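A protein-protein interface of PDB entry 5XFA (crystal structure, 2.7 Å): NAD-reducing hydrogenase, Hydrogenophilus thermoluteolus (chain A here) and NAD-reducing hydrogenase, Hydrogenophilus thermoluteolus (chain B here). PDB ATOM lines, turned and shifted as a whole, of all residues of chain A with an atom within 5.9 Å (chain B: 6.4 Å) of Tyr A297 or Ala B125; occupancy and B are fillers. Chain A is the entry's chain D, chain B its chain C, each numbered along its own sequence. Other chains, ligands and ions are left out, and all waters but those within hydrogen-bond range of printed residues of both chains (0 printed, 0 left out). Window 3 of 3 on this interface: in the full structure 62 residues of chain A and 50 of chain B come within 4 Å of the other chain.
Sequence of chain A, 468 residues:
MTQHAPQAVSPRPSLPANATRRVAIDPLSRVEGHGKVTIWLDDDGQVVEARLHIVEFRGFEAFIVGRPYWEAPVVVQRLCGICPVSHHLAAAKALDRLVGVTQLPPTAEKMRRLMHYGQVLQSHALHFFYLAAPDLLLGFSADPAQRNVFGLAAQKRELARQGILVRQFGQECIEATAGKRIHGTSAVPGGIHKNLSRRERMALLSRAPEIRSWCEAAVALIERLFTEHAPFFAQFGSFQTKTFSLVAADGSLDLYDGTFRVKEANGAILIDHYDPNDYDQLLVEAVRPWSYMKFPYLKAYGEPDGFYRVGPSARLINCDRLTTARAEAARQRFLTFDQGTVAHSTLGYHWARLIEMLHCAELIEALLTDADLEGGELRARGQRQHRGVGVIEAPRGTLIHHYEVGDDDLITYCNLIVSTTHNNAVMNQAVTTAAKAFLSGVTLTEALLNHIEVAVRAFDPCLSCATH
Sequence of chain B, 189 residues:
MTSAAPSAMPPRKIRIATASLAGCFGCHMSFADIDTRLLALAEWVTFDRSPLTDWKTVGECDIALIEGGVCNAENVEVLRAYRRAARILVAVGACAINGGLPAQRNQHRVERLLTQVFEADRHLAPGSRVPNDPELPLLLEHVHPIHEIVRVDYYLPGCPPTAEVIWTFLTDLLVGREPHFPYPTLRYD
O of His B123 sits at hydrogen-bond distance from N of Glu A285, at 2.9 Å.
The backbone carbonyl oxygen of Glu A285 sits at hydrogen-bond distance from the backbone NH of Ala B125, at 2.8 Å.
N of His B123 sits close to OD2 of Asp B121 (3.3 Å).
OG of Ser B128 lies close to N of Ala B125.
N of Tyr A297 lies within hydrogen-bond range of O of Val A284, at 2.8 Å.
Val A284 touches His B123 (CA to O, 3.5 Å).
Leu B124 touches Val A284.
Val A284 touches Ala B125 (CG1 to N, 3.5 Å).
O of Glu A285 touches CA of Leu B124, at 3.2 Å.
Val A287 touches Leu B124.
Val A287 touches Ser B128.
Tyr A297 touches Ala B125 (OH to CB, 3.7 Å).
Of the printed residues of chain B, Glu A285 touches His B123 (2.9 Å), Leu B124 (3.2 Å) and Ala B125 (2.8 Å).
Tyr A297 touches just one residue of chain B: Ala B125 (3.7 Å).
Of the printed residues of chain A, Leu B124 touches Val A284 (3.8 Å), Glu A285 (3.2 Å) and Val A287 (3.6 Å).
Of chain A, only Val A284, Glu A285 and Tyr A297 come within 4 Å of Ala B125.
The nearest residue of chain B that does not touch Tyr A297 is Pro B126 (5.4 Å).
Of the 9 printed residues of chain B, 4 touch a printed residue of chain A.
Printed residues of chain A that touch a printed residue of chain B: Val A284, Glu A285, Val A287 and Tyr A297.
Hydrophobic or aromatic side chains of chain A that line the printed part of chain B: Val A284, Val A287 and Tyr A297.
Along chain A the printed residues that touch a printed residue of chain B span positions 284 to 297.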
ATOM      1  N   LEU A 282     -24.639 -14.192   4.066  1.00  0.00           N
ATOM      2  CA  LEU A 282     -23.690 -13.390   4.789  1.00  0.00           C
ATOM      3  C   LEU A 282     -22.894 -12.474   3.857  1.00  0.00           C
ATOM      4  O   LEU A 282     -22.459 -11.381   4.262  1.00  0.00           O
ATOM      5  CB  LEU A 282     -22.747 -14.342   5.507  1.00  0.00           C
ATOM      6  CG  LEU A 282     -21.571 -13.700   6.211  1.00  0.00           C
ATOM      7  CD1 LEU A 282     -22.074 -12.742   7.275  1.00  0.00           C
ATOM      8  CD2 LEU A 282     -20.710 -14.793   6.813  1.00  0.00           C
ATOM      9  N   LEU A 283     -22.711 -12.922   2.611  1.00  0.00           N
ATOM     10  CA  LEU A 283     -21.763 -12.317   1.692  1.00  0.00           C
ATOM     11  C   LEU A 283     -22.387 -11.987   0.353  1.00  0.00           C
ATOM     12  O   LEU A 283     -23.340 -12.640  -0.080  1.00  0.00           O
ATOM     13  CB  LEU A 283     -20.619 -13.284   1.441  1.00  0.00           C
ATOM     14  CG  LEU A 283     -19.700 -13.576   2.607  1.00  0.00           C
ATOM     15  CD1 LEU A 283     -18.646 -14.554   2.125  1.00  0.00           C
ATOM     16  CD2 LEU A 283     -19.028 -12.325   3.165  1.00  0.00           C
ATOM     17  N   VAL A 284     -21.799 -10.994  -0.312  1.00  0.00           N
ATOM     18  CA  VAL A 284     -22.212 -10.568  -1.641  1.00  0.00           C
ATOM     19  C   VAL A 284     -20.981 -10.044  -2.348  1.00  0.00           C
ATOM     20  O   VAL A 284     -20.075  -9.498  -1.717  1.00  0.00           O
ATOM     21  CB  VAL A 284     -23.275  -9.448  -1.563  1.00  0.00           C
ATOM     22  CG1 VAL A 284     -23.567  -8.856  -2.930  1.00  0.00           C
ATOM     23  CG2 VAL A 284     -24.557  -9.978  -0.936  1.00  0.00           C
ATOM     24  N   GLU A 285     -20.960 -10.204  -3.664  1.00  0.00           N
ATOM     25  CA  GLU A 285     -19.809  -9.824  -4.471  1.00  0.00           C
ATOM     26  C   GLU A 285     -20.160  -8.726  -5.456  1.00  0.00           C
ATOM     27  O   GLU A 285     -21.121  -8.835  -6.210  1.00  0.00           O
ATOM     28  CB  GLU A 285     -19.294 -11.033  -5.241  1.00  0.00           C
ATOM     29  CG  GLU A 285     -18.552 -12.041  -4.383  1.00  0.00           C
ATOM     30  CD  GLU A 285     -18.112 -13.247  -5.186  1.00  0.00           C
ATOM     31  OE1 GLU A 285     -18.974 -13.834  -5.893  1.00  0.00           O
ATOM     32  OE2 GLU A 285     -16.912 -13.602  -5.102  1.00  0.00           O
ATOM     33  N   ALA A 286     -19.359  -7.676  -5.446  1.00  0.00           N
ATOM     34  CA  ALA A 286     -19.526  -6.574  -6.365  1.00  0.00           C
ATOM     35  C   ALA A 286     -18.498  -6.713  -7.479  1.00  0.00           C
ATOM     36  O   ALA A 286     -17.437  -7.304  -7.287  1.00  0.00           O
ATOM     37  CB  ALA A 286     -19.338  -5.253  -5.632  1.00  0.00           C
ATOM     38  N   VAL A 287     -18.825  -6.154  -8.635  1.00  0.00           N
ATOM     39  CA  VAL A 287     -17.971  -6.196  -9.794  1.00  0.00           C
ATOM     40  C   VAL A 287     -17.712  -4.795 -10.256  1.00  0.00           C
ATOM     41  O   VAL A 287     -18.650  -4.047 -10.534  1.00  0.00           O
ATOM     42  CB  VAL A 287     -18.666  -6.917 -10.975  1.00  0.00           C
ATOM     43  CG1 VAL A 287     -17.714  -7.068 -12.170  1.00  0.00           C
ATOM     44  CG2 VAL A 287     -19.197  -8.266 -10.529  1.00  0.00           C
ATOM     45  N   PHE A 295     -15.446  -8.165  -5.752  1.00  0.00           N
ATOM     46  CA  PHE A 295     -15.291  -7.373  -4.547  1.00  0.00           C
ATOM     47  C   PHE A 295     -16.282  -7.868  -3.523  1.00  0.00           C
ATOM     48  O   PHE A 295     -17.436  -7.438  -3.516  1.00  0.00           O
ATOM     49  CB  PHE A 295     -15.527  -5.912  -4.876  1.00  0.00           C
ATOM     50  CG  PHE A 295     -14.393  -5.285  -5.612  1.00  0.00           C
ATOM     51  CD1 PHE A 295     -14.288  -5.410  -6.984  1.00  0.00           C
ATOM     52  CD2 PHE A 295     -13.420  -4.591  -4.931  1.00  0.00           C
ATOM     53  CE1 PHE A 295     -13.225  -4.835  -7.674  1.00  0.00           C
ATOM     54  CE2 PHE A 295     -12.353  -4.025  -5.608  1.00  0.00           C
ATOM     55  CZ  PHE A 295     -12.255  -4.142  -6.984  1.00  0.00           C
ATOM     56  N   PRO A 296     -15.862  -8.825  -2.699  1.00  0.00           N
ATOM     57  CA  PRO A 296     -16.759  -9.384  -1.707  1.00  0.00           C
ATOM     58  C   PRO A 296     -16.964  -8.441  -0.535  1.00  0.00           C
ATOM     59  O   PRO A 296     -16.026  -7.755  -0.134  1.00  0.00           O
ATOM     60  CB  PRO A 296     -16.020 -10.633  -1.215  1.00  0.00           C
ATOM     61  CG  PRO A 296     -14.833 -10.795  -2.104  1.00  0.00           C
ATOM     62  CD  PRO A 296     -14.535  -9.448  -2.653  1.00  0.00           C
ATOM     63  N   TYR A 297     -18.167  -8.429   0.025  1.00  0.00           N
ATOM     64  CA  TYR A 297     -18.416  -7.684   1.247  1.00  0.00           C
ATOM     65  C   TYR A 297     -19.553  -8.305   2.032  1.00  0.00           C
ATOM     66  O   TYR A 297     -20.334  -9.128   1.509  1.00  0.00           O
ATOM     67  CB  TYR A 297     -18.704  -6.209   0.935  1.00  0.00           C
ATOM     68  CG  TYR A 297     -19.934  -5.948   0.082  1.00  0.00           C
ATOM     69  CD1 TYR A 297     -19.827  -5.690  -1.277  1.00  0.00           C
ATOM     70  CD2 TYR A 297     -21.202  -5.924   0.650  1.00  0.00           C
ATOM     71  CE1 TYR A 297     -20.952  -5.442  -2.050  1.00  0.00           C
ATOM     72  CE2 TYR A 297     -22.333  -5.684  -0.114  1.00  0.00           C
ATOM     73  CZ  TYR A 297     -22.200  -5.438  -1.462  1.00  0.00           C
ATOM     74  OH  TYR A 297     -23.326  -5.199  -2.203  1.00  0.00           O
ATOM     75  N   LEU A 298     -19.644  -7.894   3.290  1.00  0.00           N
ATOM     76  CA  LEU A 298     -20.686  -8.352   4.176  1.00  0.00           C
ATOM     77  C   LEU A 298     -22.007  -7.688   3.817  1.00  0.00           C
ATOM     78  O   LEU A 298     -22.153  -6.470   3.959  1.00  0.00           O
ATOM     79  CB  LEU A 298     -20.315  -8.043   5.611  1.00  0.00           C
ATOM     80  CG  LEU A 298     -19.162  -8.890   6.159  1.00  0.00           C
ATOM     81  CD1 LEU A 298     -18.368  -8.153   7.240  1.00  0.00           C
ATOM     82  CD2 LEU A 298     -19.686 -10.212   6.695  1.00  0.00           C
ATOM     83  N   LYS A 299     -22.963  -8.511   3.374  1.00  0.00           N
ATOM     84  CA  LYS A 299     -24.239  -8.053   2.860  1.00  0.00           C
ATOM     85  C   LYS A 299     -24.885  -6.968   3.735  1.00  0.00           C
ATOM     86  O   LYS A 299     -25.262  -5.900   3.258  1.00  0.00           O
ATOM     87  CB  LYS A 299     -25.183  -9.245   2.753  1.00  0.00           C
ATOM     88  CG  LYS A 299     -26.527  -8.925   2.133  1.00  0.00           C
ATOM     89  CD  LYS A 299     -27.190 -10.205   1.628  1.00  0.00           C
ATOM     90  CE  LYS A 299     -28.498  -9.918   0.900  1.00  0.00           C
ATOM     91  NZ  LYS A 299     -28.896 -11.018  -0.021  1.00  0.00           N
ATOM     92  N   TYR A 301     -23.884  -4.806   5.747  1.00  0.00           N
ATOM     93  CA  TYR A 301     -23.246  -3.499   5.885  1.00  0.00           C
ATOM     94  C   TYR A 301     -23.081  -2.781   4.552  1.00  0.00           C
ATOM     95  O   TYR A 301     -22.661  -1.623   4.527  1.00  0.00           O
ATOM     96  CB  TYR A 301     -21.868  -3.647   6.512  1.00  0.00           C
ATOM     97  CG  TYR A 301     -21.905  -4.190   7.902  1.00  0.00           C
ATOM     98  CD1 TYR A 301     -22.284  -5.504   8.136  1.00  0.00           C
ATOM     99  CD2 TYR A 301     -21.568  -3.398   9.001  1.00  0.00           C
ATOM    100  CE1 TYR A 301     -22.327  -6.026   9.417  1.00  0.00           C
ATOM    101  CE2 TYR A 301     -21.612  -3.909  10.295  1.00  0.00           C
ATOM    102  CZ  TYR A 301     -21.996  -5.228  10.493  1.00  0.00           C
ATOM    103  OH  TYR A 301     -22.058  -5.781  11.749  1.00  0.00           O
ATOM    104  N   GLY A 302     -23.388  -3.452   3.444  1.00  0.00           N
ATOM    105  CA  GLY A 302     -23.119  -2.898   2.119  1.00  0.00           C
ATOM    106  C   GLY A 302     -21.671  -2.462   1.979  1.00  0.00           C
ATOM    107  O   GLY A 302     -20.824  -2.819   2.810  1.00  0.00           O
ATOM    108  N   GLU A 303     -21.386  -1.674   0.948  1.00  0.00           N
ATOM    109  CA  GLU A 303     -20.024  -1.184   0.716  1.00  0.00           C
ATOM    110  C   GLU A 303     -19.991   0.323   0.850  1.00  0.00           C
ATOM    111  O   GLU A 303     -20.941   0.981   0.459  1.00  0.00           O
ATOM    112  CB  GLU A 303     -19.514  -1.599  -0.662  1.00  0.00           C
ATOM    113  CG  GLU A 303     -20.424  -1.244  -1.820  1.00  0.00           C
ATOM    114  CD  GLU A 303     -19.935  -1.817  -3.142  1.00  0.00           C
ATOM    115  OE1 GLU A 303     -18.892  -1.351  -3.648  1.00  0.00           O
ATOM    116  OE2 GLU A 303     -20.617  -2.719  -3.684  1.00  0.00           O
ATOM    117  N   GLY A 306     -18.972  -2.808   4.608  1.00  0.00           N
ATOM    118  CA  GLY A 306     -18.933  -4.279   4.666  1.00  0.00           C
ATOM    119  C   GLY A 306     -17.699  -4.973   4.107  1.00  0.00           C
ATOM    120  O   GLY A 306     -17.662  -6.202   4.051  1.00  0.00           O
ATOM    121  N   PHE A 307     -16.702  -4.217   3.660  1.00  0.00           N
ATOM    122  CA  PHE A 307     -15.457  -4.829   3.225  1.00  0.00           C
ATOM    123  C   PHE A 307     -14.720  -5.350   4.437  1.00  0.00           C
ATOM    124  O   PHE A 307     -14.969  -4.898   5.544  1.00  0.00           O
ATOM    125  CB  PHE A 307     -14.568  -3.857   2.442  1.00  0.00           C
ATOM    126  CG  PHE A 307     -15.056  -3.566   1.057  1.00  0.00           C
ATOM    127  CD1 PHE A 307     -15.487  -4.585   0.235  1.00  0.00           C
ATOM    128  CD2 PHE A 307     -15.049  -2.278   0.567  1.00  0.00           C
ATOM    129  CE1 PHE A 307     -15.929  -4.327  -1.051  1.00  0.00           C
ATOM    130  CE2 PHE A 307     -15.481  -2.005  -0.714  1.00  0.00           C
ATOM    131  CZ  PHE A 307     -15.924  -3.033  -1.528  1.00  0.00           C
ATOM    132  N   TYR A 308     -13.825  -6.305   4.202  1.00  0.00           N
ATOM    133  CA  TYR A 308     -13.008  -6.887   5.258  1.00  0.00           C
ATOM    134  C   TYR A 308     -11.681  -7.370   4.671  1.00  0.00           C
ATOM    135  O   TYR A 308     -11.377  -7.130   3.498  1.00  0.00           O
ATOM    136  CB  TYR A 308     -13.751  -8.026   5.923  1.00  0.00           C
ATOM    137  CG  TYR A 308     -14.314  -8.979   4.920  1.00  0.00           C
ATOM    138  CD1 TYR A 308     -13.551 -10.003   4.395  1.00  0.00           C
ATOM    139  CD2 TYR A 308     -15.609  -8.845   4.490  1.00  0.00           C
ATOM    140  CE1 TYR A 308     -14.078 -10.875   3.479  1.00  0.00           C
ATOM    141  CE2 TYR A 308     -16.156  -9.719   3.571  1.00  0.00           C
ATOM    142  CZ  TYR A 308     -15.389 -10.730   3.065  1.00  0.00           C
ATOM    143  OH  TYR A 308     -15.948 -11.580   2.126  1.00  0.00           O
ATOM    144  N   GLU B 119     -22.630 -11.383 -14.273  1.00  0.00           N
ATOM    145  CA  GLU B 119     -23.964 -10.787 -14.318  1.00  0.00           C
ATOM    146  C   GLU B 119     -25.044 -11.648 -13.698  1.00  0.00           C
ATOM    147  O   GLU B 119     -25.882 -11.145 -12.941  1.00  0.00           O
ATOM    148  CB  GLU B 119     -24.360 -10.437 -15.755  1.00  0.00           C
ATOM    149  CG  GLU B 119     -23.499  -9.338 -16.383  1.00  0.00           C
ATOM    150  CD  GLU B 119     -24.050  -8.782 -17.695  1.00  0.00           C
ATOM    151  OE1 GLU B 119     -25.203  -9.132 -18.054  1.00  0.00           O
ATOM    152  OE2 GLU B 119     -23.319  -8.011 -18.375  1.00  0.00           O
ATOM    153  N   ASP B 121     -24.865 -14.382 -11.648  1.00  0.00           N
ATOM    154  CA  ASP B 121     -24.636 -15.157 -10.452  1.00  0.00           C
ATOM    155  C   ASP B 121     -25.464 -14.610  -9.305  1.00  0.00           C
ATOM    156  O   ASP B 121     -25.336 -13.440  -8.938  1.00  0.00           O
ATOM    157  CB  ASP B 121     -23.152 -15.152 -10.083  1.00  0.00           C
ATOM    158  CG  ASP B 121     -22.838 -16.067  -8.920  1.00  0.00           C
ATOM    159  OD1 ASP B 121     -23.044 -17.296  -9.084  1.00  0.00           O
ATOM    160  OD2 ASP B 121     -22.381 -15.554  -7.862  1.00  0.00           O
ATOM    161  N   ARG B 122     -26.283 -15.483  -8.724  1.00  0.00           N
ATOM    162  CA  ARG B 122     -27.136 -15.138  -7.585  1.00  0.00           C
ATOM    163  C   ARG B 122     -26.445 -14.384  -6.441  1.00  0.00           C
ATOM    164  O   ARG B 122     -27.116 -13.715  -5.694  1.00  0.00           O
ATOM    165  CB  ARG B 122     -27.797 -16.395  -7.011  1.00  0.00           C
ATOM    166  CG  ARG B 122     -26.821 -17.318  -6.305  1.00  0.00           C
ATOM    167  CD  ARG B 122     -27.457 -18.649  -5.949  1.00  0.00           C
ATOM    168  NE  ARG B 122     -27.446 -19.571  -7.090  1.00  0.00           N
ATOM    169  CZ  ARG B 122     -27.656 -20.886  -7.018  1.00  0.00           C
ATOM    170  NH1 ARG B 122     -27.895 -21.480  -5.852  1.00  0.00           N
ATOM    171  NH2 ARG B 122     -27.615 -21.620  -8.121  1.00  0.00           N
ATOM    172  N   HIS B 123     -25.134 -14.497  -6.288  1.00  0.00           N
ATOM    173  CA  HIS B 123     -24.446 -13.824  -5.172  1.00  0.00           C
ATOM    174  C   HIS B 123     -23.822 -12.499  -5.549  1.00  0.00           C
ATOM    175  O   HIS B 123     -23.016 -11.973  -4.779  1.00  0.00           O
ATOM    176  CB  HIS B 123     -23.349 -14.722  -4.575  1.00  0.00           C
ATOM    177  CG  HIS B 123     -23.770 -16.141  -4.420  1.00  0.00           C
ATOM    178  ND1 HIS B 123     -24.435 -16.611  -3.311  1.00  0.00           N
ATOM    179  CD2 HIS B 123     -23.660 -17.183  -5.267  1.00  0.00           C
ATOM    180  CE1 HIS B 123     -24.706 -17.891  -3.476  1.00  0.00           C
ATOM    181  NE2 HIS B 123     -24.253 -18.260  -4.661  1.00  0.00           N
ATOM    182  N   LEU B 124     -24.155 -11.966  -6.724  1.00  0.00           N
ATOM    183  CA  LEU B 124     -23.633 -10.664  -7.109  1.00  0.00           C
ATOM    184  C   LEU B 124     -24.489  -9.557  -6.541  1.00  0.00           C
ATOM    185  O   LEU B 124     -25.652  -9.749  -6.232  1.00  0.00           O
ATOM    186  CB  LEU B 124     -23.586 -10.523  -8.616  1.00  0.00           C
ATOM    187  CG  LEU B 124     -22.596 -11.423  -9.331  1.00  0.00           C
ATOM    188  CD1 LEU B 124     -22.898 -11.439 -10.816  1.00  0.00           C
ATOM    189  CD2 LEU B 124     -21.176 -10.956  -9.085  1.00  0.00           C
ATOM    190  N   ALA B 125     -23.891  -8.384  -6.416  1.00  0.00           N
ATOM    191  CA  ALA B 125     -24.616  -7.168  -6.080  1.00  0.00           C
ATOM    192  C   ALA B 125     -25.563  -6.831  -7.235  1.00  0.00           C
ATOM    193  O   ALA B 125     -25.297  -7.199  -8.392  1.00  0.00           O
ATOM    194  CB  ALA B 125     -23.647  -6.021  -5.846  1.00  0.00           C
ATOM    195  N   PRO B 126     -26.688  -6.164  -6.925  1.00  0.00           N
ATOM    196  CA  PRO B 126     -27.514  -5.632  -8.004  1.00  0.00           C
ATOM    197  C   PRO B 126     -26.747  -4.673  -8.928  1.00  0.00           C
ATOM    198  O   PRO B 126     -25.930  -3.881  -8.460  1.00  0.00           O
ATOM    199  CB  PRO B 126     -28.633  -4.912  -7.251  1.00  0.00           C
ATOM    200  CG  PRO B 126     -28.799  -5.721  -6.000  1.00  0.00           C
ATOM    201  CD  PRO B 126     -27.413  -6.185  -5.640  1.00  0.00           C
ATOM    202  N   GLY B 127     -26.998  -4.797 -10.229  1.00  0.00           N
ATOM    203  CA  GLY B 127     -26.367  -3.962 -11.257  1.00  0.00           C
ATOM    204  C   GLY B 127     -25.046  -4.480 -11.825  1.00  0.00           C
ATOM    205  O   GLY B 127     -24.430  -3.811 -12.650  1.00  0.00           O
ATOM    206  N   SER B 128     -24.619  -5.676 -11.416  1.00  0.00           N
ATOM    207  CA  SER B 128     -23.288  -6.155 -11.755  1.00  0.00           C
ATOM    208  C   SER B 128     -23.191  -6.468 -13.223  1.00  0.00           C
ATOM    209  O   SER B 128     -24.063  -7.136 -13.755  1.00  0.00           O
ATOM    210  CB  SER B 128     -22.970  -7.406 -10.958  1.00  0.00           C
ATOM    211  OG  SER B 128     -23.303  -7.211  -9.602  1.00  0.00           O
